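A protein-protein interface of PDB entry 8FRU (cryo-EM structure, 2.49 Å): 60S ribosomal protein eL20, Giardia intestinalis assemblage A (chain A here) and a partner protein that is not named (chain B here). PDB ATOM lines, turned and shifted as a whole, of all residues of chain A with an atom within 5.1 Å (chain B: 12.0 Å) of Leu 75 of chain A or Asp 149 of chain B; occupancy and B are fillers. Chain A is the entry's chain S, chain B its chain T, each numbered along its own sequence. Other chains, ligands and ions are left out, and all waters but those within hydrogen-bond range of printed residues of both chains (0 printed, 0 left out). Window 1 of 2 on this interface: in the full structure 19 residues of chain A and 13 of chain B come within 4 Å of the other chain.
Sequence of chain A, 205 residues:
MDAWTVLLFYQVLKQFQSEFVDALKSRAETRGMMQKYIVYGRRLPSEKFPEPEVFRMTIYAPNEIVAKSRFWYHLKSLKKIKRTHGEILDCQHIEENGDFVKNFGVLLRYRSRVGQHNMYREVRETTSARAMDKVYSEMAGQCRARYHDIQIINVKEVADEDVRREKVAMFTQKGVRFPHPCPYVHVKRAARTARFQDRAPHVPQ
The guanidinium group (NH2) of Arg 56 of chain A lies within hydrogen-bond range of the side-chain hydroxyl (OG) of Ser 146 of chain B, at 3.5 Å.
O of Ala 147 of chain B is in hydrogen-bond range of N of Arg 56 of chain A.
The backbone NH of Asp 149 of chain B sits at hydrogen-bond distance from the backbone carbonyl oxygen of Arg 56 of chain A (2.9 Å).
The backbone carbonyl oxygen of Leu 75 of chain A is in hydrogen-bond range of the backbone NH of Lys 80 of chain A (3.4 Å).
CA of Phe 55 of chain A touches O of Ala 147 of chain B, 3.5 Å away.
Asp 149 of chain B touches Phe 55 of chain A (OD1 to CD1, 3.6 Å).
Ile 148 of chain B touches Arg 56 of chain A (CG1 to NH1, 3.3 Å).
O of Asp 149 of chain B touches CG of Met 57 of chain A, 3.5 Å away.
His 74 of chain A touches Thr 151 of chain B (CE1 to CG2, 3.6 Å).
Leu 75 of chain A touches Asp 149 of chain B (CD1 to OD1, 3.7 Å).
Leu 78 of chain A touches Ile 150 of chain B.
Lys 79 of chain A touches Asp 149 of chain B.
Phe 55 of chain A touches just these residues of chain B: Ala 147 and Asp 149.
Met 57 of chain A touches one residue of chain B.
No residue of chain B comes within 4 Å of Phe 71 of chain A.
No residue of chain B comes within 4 Å of Trp 72 of chain A.
Of chain B, only Thr 151 (3.6 Å) comes within 4 Å of His 74 of chain A.
Leu 75 of chain A touches just one residue of chain B: Asp 149 (3.7 Å).
Lys 76 of chain A touches none of the printed residues of chain B.
Of chain B, only Ile 150 (3.1 Å) comes within 4 Å of Leu 78 of chain A.
Printed residues of chain B within 4 Å of Lys 79 of chain A: Asp 149 (3.7 Å).
Of the printed residues of chain A, Ser 146 of chain B touches Arg 56 (3.5 Å).
Of the printed residues of chain A, Ala 147 of chain B touches Phe 55 (3.5 Å) and Arg 56 (3.3 Å).
Of the printed residues of chain A, Asp 149 of chain B touches Phe 55 (3.6 Å), Arg 56 (2.9 Å), Met 57 (3.5 Å), Leu 75 (3.7 Å) and Lys 79 (3.7 Å).
The nearest residue of chain B that does not touch Leu 75 of chain A is Ala 147 of chain B (7.8 Å).
Hydrophobic or aromatic side chains of chain A that line the printed part of chain B: Phe 55, Met 57, His 74, Leu 75 and Leu 78.
Of the 11 printed residues of chain B, 6 touch a printed residue of chain A.
Along chain B the printed residues that touch a printed residue of chain A span positions 146 to 151.
Among the printed residues, 11 pairs touch across the chains.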
ATOM      1  N   PHE A  55     -21.511  -1.943  -8.453  1.00  0.00           N
ATOM      2  CA  PHE A  55     -22.130  -2.836  -7.486  1.00  0.00           C
ATOM      3  C   PHE A  55     -23.631  -2.879  -7.717  1.00  0.00           C
ATOM      4  O   PHE A  55     -24.250  -1.856  -8.017  1.00  0.00           O
ATOM      5  CB  PHE A  55     -21.832  -2.392  -6.057  1.00  0.00           C
ATOM      6  CG  PHE A  55     -20.370  -2.269  -5.763  1.00  0.00           C
ATOM      7  CD1 PHE A  55     -19.595  -3.392  -5.561  1.00  0.00           C
ATOM      8  CD2 PHE A  55     -19.769  -1.030  -5.696  1.00  0.00           C
ATOM      9  CE1 PHE A  55     -18.256  -3.279  -5.303  1.00  0.00           C
ATOM     10  CE2 PHE A  55     -18.432  -0.915  -5.432  1.00  0.00           C
ATOM     11  CZ  PHE A  55     -17.673  -2.040  -5.235  1.00  0.00           C
ATOM     12  N   ARG A  56     -24.205  -4.068  -7.583  1.00  0.00           N
ATOM     13  CA  ARG A  56     -25.634  -4.286  -7.748  1.00  0.00           C
ATOM     14  C   ARG A  56     -26.205  -4.915  -6.485  1.00  0.00           C
ATOM     15  O   ARG A  56     -25.581  -5.791  -5.884  1.00  0.00           O
ATOM     16  CB  ARG A  56     -25.924  -5.190  -8.947  1.00  0.00           C
ATOM     17  CG  ARG A  56     -27.394  -5.501  -9.106  1.00  0.00           C
ATOM     18  CD  ARG A  56     -27.649  -6.895  -9.651  1.00  0.00           C
ATOM     19  NE  ARG A  56     -27.282  -7.042 -11.053  1.00  0.00           N
ATOM     20  CZ  ARG A  56     -26.189  -7.654 -11.486  1.00  0.00           C
ATOM     21  NH1 ARG A  56     -25.322  -8.199 -10.649  1.00  0.00           N
ATOM     22  NH2 ARG A  56     -25.963  -7.728 -12.795  1.00  0.00           N
ATOM     23  N   MET A  57     -27.393  -4.465  -6.089  1.00  0.00           N
ATOM     24  CA  MET A  57     -28.068  -4.989  -4.911  1.00  0.00           C
ATOM     25  C   MET A  57     -29.562  -5.082  -5.181  1.00  0.00           C
ATOM     26  O   MET A  57     -30.099  -4.402  -6.056  1.00  0.00           O
ATOM     27  CB  MET A  57     -27.811  -4.116  -3.678  1.00  0.00           C
ATOM     28  CG  MET A  57     -27.934  -4.862  -2.365  1.00  0.00           C
ATOM     29  SD  MET A  57     -27.127  -4.054  -0.971  1.00  0.00           S
ATOM     30  CE  MET A  57     -25.988  -2.970  -1.816  1.00  0.00           C
ATOM     31  N   ARG A  70     -31.564   2.853   1.594  1.00  0.00           N
ATOM     32  CA  ARG A  70     -31.038   1.580   2.080  1.00  0.00           C
ATOM     33  C   ARG A  70     -29.832   1.122   1.270  1.00  0.00           C
ATOM     34  O   ARG A  70     -28.893   0.530   1.818  1.00  0.00           O
ATOM     35  CB  ARG A  70     -32.132   0.519   2.058  1.00  0.00           C
ATOM     36  CG  ARG A  70     -33.153   0.675   3.160  1.00  0.00           C
ATOM     37  CD  ARG A  70     -32.805  -0.181   4.359  1.00  0.00           C
ATOM     38  NE  ARG A  70     -32.310   0.618   5.470  1.00  0.00           N
ATOM     39  CZ  ARG A  70     -31.915   0.123   6.634  1.00  0.00           C
ATOM     40  NH1 ARG A  70     -31.946  -1.176   6.877  1.00  0.00           N
ATOM     41  NH2 ARG A  70     -31.478   0.952   7.576  1.00  0.00           N
ATOM     42  N   PHE A  71     -29.840   1.377  -0.037  1.00  0.00           N
ATOM     43  CA  PHE A  71     -28.672   1.054  -0.847  1.00  0.00           C
ATOM     44  C   PHE A  71     -27.434   1.752  -0.310  1.00  0.00           C
ATOM     45  O   PHE A  71     -26.390   1.123  -0.104  1.00  0.00           O
ATOM     46  CB  PHE A  71     -28.908   1.447  -2.302  1.00  0.00           C
ATOM     47  CG  PHE A  71     -27.721   1.210  -3.183  1.00  0.00           C
ATOM     48  CD1 PHE A  71     -27.417  -0.059  -3.630  1.00  0.00           C
ATOM     49  CD2 PHE A  71     -26.898   2.255  -3.549  1.00  0.00           C
ATOM     50  CE1 PHE A  71     -26.322  -0.280  -4.431  1.00  0.00           C
ATOM     51  CE2 PHE A  71     -25.802   2.038  -4.349  1.00  0.00           C
ATOM     52  CZ  PHE A  71     -25.514   0.770  -4.790  1.00  0.00           C
ATOM     53  N   TRP A  72     -27.530   3.061  -0.084  1.00  0.00           N
ATOM     54  CA  TRP A  72     -26.381   3.791   0.439  1.00  0.00           C
ATOM     55  C   TRP A  72     -26.021   3.328   1.838  1.00  0.00           C
ATOM     56  O   TRP A  72     -24.839   3.279   2.189  1.00  0.00           O
ATOM     57  CB  TRP A  72     -26.656   5.288   0.416  1.00  0.00           C
ATOM     58  CG  TRP A  72     -26.523   5.855  -0.942  1.00  0.00           C
ATOM     59  CD1 TRP A  72     -27.486   6.476  -1.666  1.00  0.00           C
ATOM     60  CD2 TRP A  72     -25.353   5.838  -1.761  1.00  0.00           C
ATOM     61  NE1 TRP A  72     -26.992   6.855  -2.884  1.00  0.00           N
ATOM     62  CE2 TRP A  72     -25.680   6.473  -2.967  1.00  0.00           C
ATOM     63  CE3 TRP A  72     -24.058   5.350  -1.587  1.00  0.00           C
ATOM     64  CZ2 TRP A  72     -24.761   6.638  -3.991  1.00  0.00           C
ATOM     65  CZ3 TRP A  72     -23.153   5.509  -2.606  1.00  0.00           C
ATOM     66  CH2 TRP A  72     -23.505   6.149  -3.792  1.00  0.00           C
ATOM     67  N   TYR A  73     -27.020   2.959   2.638  1.00  0.00           N
ATOM     68  CA  TYR A  73     -26.750   2.443   3.972  1.00  0.00           C
ATOM     69  C   TYR A  73     -25.858   1.212   3.915  1.00  0.00           C
ATOM     70  O   TYR A  73     -24.904   1.088   4.688  1.00  0.00           O
ATOM     71  CB  TYR A  73     -28.067   2.122   4.678  1.00  0.00           C
ATOM     72  CG  TYR A  73     -27.901   1.426   6.005  1.00  0.00           C
ATOM     73  CD1 TYR A  73     -27.832   0.046   6.083  1.00  0.00           C
ATOM     74  CD2 TYR A  73     -27.810   2.150   7.179  1.00  0.00           C
ATOM     75  CE1 TYR A  73     -27.676  -0.589   7.290  1.00  0.00           C
ATOM     76  CE2 TYR A  73     -27.658   1.524   8.389  1.00  0.00           C
ATOM     77  CZ  TYR A  73     -27.594   0.155   8.440  1.00  0.00           C
ATOM     78  OH  TYR A  73     -27.440  -0.472   9.649  1.00  0.00           O
ATOM     79  N   HIS A  74     -26.157   0.282   3.012  1.00  0.00           N
ATOM     80  CA  HIS A  74     -25.340  -0.927   2.939  1.00  0.00           C
ATOM     81  C   HIS A  74     -24.005  -0.682   2.251  1.00  0.00           C
ATOM     82  O   HIS A  74     -22.990  -1.277   2.633  1.00  0.00           O
ATOM     83  CB  HIS A  74     -26.101  -2.048   2.238  1.00  0.00           C
ATOM     84  CG  HIS A  74     -27.212  -2.617   3.057  1.00  0.00           C
ATOM     85  ND1 HIS A  74     -26.994  -3.263   4.254  1.00  0.00           N
ATOM     86  CD2 HIS A  74     -28.550  -2.642   2.855  1.00  0.00           C
ATOM     87  CE1 HIS A  74     -28.148  -3.661   4.753  1.00  0.00           C
ATOM     88  NE2 HIS A  74     -29.108  -3.297   3.923  1.00  0.00           N
ATOM     89  N   LEU A  75     -23.975   0.188   1.243  1.00  0.00           N
ATOM     90  CA  LEU A  75     -22.723   0.443   0.543  1.00  0.00           C
ATOM     91  C   LEU A  75     -21.717   1.143   1.445  1.00  0.00           C
ATOM     92  O   LEU A  75     -20.512   0.906   1.333  1.00  0.00           O
ATOM     93  CB  LEU A  75     -22.974   1.264  -0.717  1.00  0.00           C
ATOM     94  CG  LEU A  75     -21.910   1.119  -1.801  1.00  0.00           C
ATOM     95  CD1 LEU A  75     -21.881  -0.297  -2.320  1.00  0.00           C
ATOM     96  CD2 LEU A  75     -22.161   2.089  -2.925  1.00  0.00           C
ATOM     97  N   LYS A  76     -22.186   2.020   2.333  1.00  0.00           N
ATOM     98  CA  LYS A  76     -21.267   2.683   3.251  1.00  0.00           C
ATOM     99  C   LYS A  76     -20.602   1.679   4.182  1.00  0.00           C
ATOM    100  O   LYS A  76     -19.395   1.756   4.430  1.00  0.00           O
ATOM    101  CB  LYS A  76     -22.009   3.752   4.051  1.00  0.00           C
ATOM    102  CG  LYS A  76     -21.101   4.823   4.621  1.00  0.00           C
ATOM    103  CD  LYS A  76     -21.795   5.684   5.662  1.00  0.00           C
ATOM    104  CE  LYS A  76     -21.948   4.955   6.976  1.00  0.00           C
ATOM    105  NZ  LYS A  76     -22.178   5.898   8.101  1.00  0.00           N
ATOM    106  N   SER A  77     -21.372   0.727   4.701  1.00  0.00           N
ATOM    107  CA  SER A  77     -20.849  -0.224   5.672  1.00  0.00           C
ATOM    108  C   SER A  77     -20.002  -1.313   5.034  1.00  0.00           C
ATOM    109  O   SER A  77     -19.038  -1.772   5.648  1.00  0.00           O
ATOM    110  CB  SER A  77     -21.997  -0.862   6.448  1.00  0.00           C
ATOM    111  OG  SER A  77     -23.108   0.007   6.492  1.00  0.00           O
ATOM    112  N   LEU A  78     -20.343  -1.757   3.826  1.00  0.00           N
ATOM    113  CA  LEU A  78     -19.643  -2.888   3.235  1.00  0.00           C
ATOM    114  C   LEU A  78     -18.495  -2.492   2.326  1.00  0.00           C
ATOM    115  O   LEU A  78     -17.535  -3.254   2.204  1.00  0.00           O
ATOM    116  CB  LEU A  78     -20.617  -3.767   2.446  1.00  0.00           C
ATOM    117  CG  LEU A  78     -21.797  -4.328   3.234  1.00  0.00           C
ATOM    118  CD1 LEU A  78     -22.867  -4.833   2.296  1.00  0.00           C
ATOM    119  CD2 LEU A  78     -21.338  -5.426   4.163  1.00  0.00           C
ATOM    120  N   LYS A  79     -18.554  -1.328   1.693  1.00  0.00           N
ATOM    121  CA  LYS A  79     -17.532  -0.946   0.736  1.00  0.00           C
ATOM    122  C   LYS A  79     -16.890   0.398   1.026  1.00  0.00           C
ATOM    123  O   LYS A  79     -16.073   0.854   0.223  1.00  0.00           O
ATOM    124  CB  LYS A  79     -18.112  -0.926  -0.683  1.00  0.00           C
ATOM    125  CG  LYS A  79     -18.471  -2.294  -1.217  1.00  0.00           C
ATOM    126  CD  LYS A  79     -17.233  -3.126  -1.461  1.00  0.00           C
ATOM    127  CE  LYS A  79     -17.582  -4.466  -2.073  1.00  0.00           C
ATOM    128  NZ  LYS A  79     -16.382  -5.319  -2.269  1.00  0.00           N
ATOM    129  N   LYS A  80     -17.231   1.045   2.138  1.00  0.00           N
ATOM    130  CA  LYS A  80     -16.613   2.312   2.521  1.00  0.00           C
ATOM    131  C   LYS A  80     -16.839   3.390   1.464  1.00  0.00           C
ATOM    132  O   LYS A  80     -15.940   4.167   1.148  1.00  0.00           O
ATOM    133  CB  LYS A  80     -15.122   2.122   2.792  1.00  0.00           C
ATOM    134  CG  LYS A  80     -14.505   3.161   3.692  1.00  0.00           C
ATOM    135  CD  LYS A  80     -13.008   2.966   3.780  1.00  0.00           C
ATOM    136  CE  LYS A  80     -12.423   3.623   5.010  1.00  0.00           C
ATOM    137  NZ  LYS A  80     -12.923   2.991   6.248  1.00  0.00           N
ATOM    138  N   ILE A  81     -18.048   3.444   0.914  1.00  0.00           N
ATOM    139  CA  ILE A  81     -18.441   4.472  -0.041  1.00  0.00           C
ATOM    140  C   ILE A  81     -19.667   5.181   0.509  1.00  0.00           C
ATOM    141  O   ILE A  81     -20.700   4.547   0.744  1.00  0.00           O
ATOM    142  CB  ILE A  81     -18.728   3.886  -1.432  1.00  0.00           C
ATOM    143  CG1 ILE A  81     -17.544   3.047  -1.908  1.00  0.00           C
ATOM    144  CG2 ILE A  81     -19.033   4.989  -2.428  1.00  0.00           C
ATOM    145  CD1 ILE A  81     -17.809   2.281  -3.168  1.00  0.00           C
ATOM    146  N   ARG B 137     -24.277  16.873 -12.269  1.00  0.00           N
ATOM    147  CA  ARG B 137     -23.599  16.102 -13.300  1.00  0.00           C
ATOM    148  C   ARG B 137     -24.473  15.959 -14.544  1.00  0.00           C
ATOM    149  O   ARG B 137     -25.699  16.078 -14.498  1.00  0.00           O
ATOM    150  CB  ARG B 137     -23.210  14.725 -12.764  1.00  0.00           C
ATOM    151  CG  ARG B 137     -22.072  14.772 -11.764  1.00  0.00           C
ATOM    152  CD  ARG B 137     -21.649  13.392 -11.303  1.00  0.00           C
ATOM    153  NE  ARG B 137     -22.249  13.036 -10.023  1.00  0.00           N
ATOM    154  CZ  ARG B 137     -23.387  12.371  -9.886  1.00  0.00           C
ATOM    155  NH1 ARG B 137     -24.070  11.948 -10.937  1.00  0.00           N
ATOM    156  NH2 ARG B 137     -23.851  12.123  -8.665  1.00  0.00           N
ATOM    157  N   ILE B 144     -21.266  -2.272 -17.779  1.00  0.00           N
ATOM    158  CA  ILE B 144     -21.636  -3.145 -16.674  1.00  0.00           C
ATOM    159  C   ILE B 144     -20.736  -4.375 -16.679  1.00  0.00           C
ATOM    160  O   ILE B 144     -20.746  -5.161 -17.636  1.00  0.00           O
ATOM    161  CB  ILE B 144     -23.112  -3.556 -16.745  1.00  0.00           C
ATOM    162  CG1 ILE B 144     -23.982  -2.540 -16.011  1.00  0.00           C
ATOM    163  CG2 ILE B 144     -23.294  -4.936 -16.156  1.00  0.00           C
ATOM    164  CD1 ILE B 144     -25.422  -2.556 -16.448  1.00  0.00           C
ATOM    165  N   ALA B 145     -19.959  -4.533 -15.609  1.00  0.00           N
ATOM    166  CA  ALA B 145     -19.270  -5.775 -15.259  1.00  0.00           C
ATOM    167  C   ALA B 145     -19.441  -6.001 -13.761  1.00  0.00           C
ATOM    168  O   ALA B 145     -18.508  -6.357 -13.042  1.00  0.00           O
ATOM    169  CB  ALA B 145     -17.794  -5.731 -15.650  1.00  0.00           C
ATOM    170  N   SER B 146     -20.668  -5.795 -13.290  1.00  0.00           N
ATOM    171  CA  SER B 146     -20.943  -5.519 -11.891  1.00  0.00           C
ATOM    172  C   SER B 146     -20.710  -6.737 -11.007  1.00  0.00           C
ATOM    173  O   SER B 146     -20.708  -7.885 -11.457  1.00  0.00           O
ATOM    174  CB  SER B 146     -22.379  -5.034 -11.727  1.00  0.00           C
ATOM    175  OG  SER B 146     -23.209  -5.583 -12.729  1.00  0.00           O
ATOM    176  N   ALA B 147     -20.518  -6.459  -9.723  1.00  0.00           N
ATOM    177  CA  ALA B 147     -20.360  -7.472  -8.692  1.00  0.00           C
ATOM    178  C   ALA B 147     -21.543  -7.392  -7.739  1.00  0.00           C
ATOM    179  O   ALA B 147     -21.842  -6.321  -7.206  1.00  0.00           O
ATOM    180  CB  ALA B 147     -19.047  -7.274  -7.930  1.00  0.00           C
ATOM    181  N   ILE B 148     -22.211  -8.524  -7.528  1.00  0.00           N
ATOM    182  CA  ILE B 148     -23.354  -8.570  -6.624  1.00  0.00           C
ATOM    183  C   ILE B 148     -22.896  -8.319  -5.194  1.00  0.00           C
ATOM    184  O   ILE B 148     -21.925  -8.919  -4.718  1.00  0.00           O
ATOM    185  CB  ILE B 148     -24.078  -9.917  -6.745  1.00  0.00           C
ATOM    186  CG1 ILE B 148     -25.154  -9.849  -7.824  1.00  0.00           C
ATOM    187  CG2 ILE B 148     -24.673 -10.317  -5.412  1.00  0.00           C
ATOM    188  CD1 ILE B 148     -26.383  -9.081  -7.405  1.00  0.00           C
ATOM    189  N   ASP B 149     -23.605  -7.437  -4.501  1.00  0.00           N
ATOM    190  CA  ASP B 149     -23.313  -7.080  -3.123  1.00  0.00           C
ATOM    191  C   ASP B 149     -24.426  -7.576  -2.214  1.00  0.00           C
ATOM    192  O   ASP B 149     -25.608  -7.469  -2.550  1.00  0.00           O
ATOM    193  CB  ASP B 149     -23.159  -5.570  -2.973  1.00  0.00           C
ATOM    194  CG  ASP B 149     -21.746  -5.165  -2.670  1.00  0.00           C
ATOM    195  OD1 ASP B 149     -21.501  -3.955  -2.508  1.00  0.00           O
ATOM    196  OD2 ASP B 149     -20.878  -6.056  -2.594  1.00  0.00           O
ATOM    197  N   ILE B 150     -24.043  -8.115  -1.058  1.00  0.00           N
ATOM    198  CA  ILE B 150     -24.978  -8.706  -0.111  1.00  0.00           C
ATOM    199  C   ILE B 150     -24.599  -8.269   1.300  1.00  0.00           C
ATOM    200  O   ILE B 150     -23.520  -7.730   1.544  1.00  0.00           O
ATOM    201  CB  ILE B 150     -25.007 -10.245  -0.214  1.00  0.00           C
ATOM    202  CG1 ILE B 150     -26.254 -10.810   0.462  1.00  0.00           C
ATOM    203  CG2 ILE B 150     -23.746 -10.845   0.378  1.00  0.00           C
ATOM    204  CD1 ILE B 150     -27.389 -11.084  -0.492  1.00  0.00           C
ATOM    205  N   THR B 151     -25.502  -8.522   2.229  1.00  0.00           N
ATOM    206  CA  THR B 151     -25.398  -8.172   3.639  1.00  0.00           C
ATOM    207  C   THR B 151     -24.870  -9.353   4.439  1.00  0.00           C
ATOM    208  O   THR B 151     -25.364 -10.474   4.264  1.00  0.00           O
ATOM    209  CB  THR B 151     -26.763  -7.755   4.171  1.00  0.00           C
ATOM    210  OG1 THR B 151     -27.483  -7.077   3.138  1.00  0.00           O
ATOM    211  CG2 THR B 151     -26.610  -6.836   5.337  1.00  0.00           C
ATOM    212  N   PRO B 152     -23.872  -9.165   5.298  1.00  0.00           N
ATOM    213  CA  PRO B 152     -23.294 -10.305   6.023  1.00  0.00           C
ATOM    214  C   PRO B 152     -24.078 -10.648   7.283  1.00  0.00           C
ATOM    215  O   PRO B 152     -24.916  -9.891   7.771  1.00  0.00           O
ATOM    216  CB  PRO B 152     -21.877  -9.832   6.358  1.00  0.00           C
ATOM    217  N   LEU B 153     -23.777 -11.828   7.818  1.00  0.00           N
ATOM    218  CA  LEU B 153     -24.362 -12.292   9.065  1.00  0.00           C
ATOM    219  C   LEU B 153     -23.715 -11.563  10.238  1.00  0.00           C
ATOM    220  O   LEU B 153     -22.693 -10.890  10.096  1.00  0.00           O
ATOM    221  CB  LEU B 153     -24.194 -13.805   9.189  1.00  0.00           C
ATOM    222  CG  LEU B 153     -25.270 -14.664   8.516  1.00  0.00           C
ATOM    223  CD1 LEU B 153     -24.923 -14.917   7.061  1.00  0.00           C
ATOM    224  CD2 LEU B 153     -25.455 -15.983   9.243  1.00  0.00           C
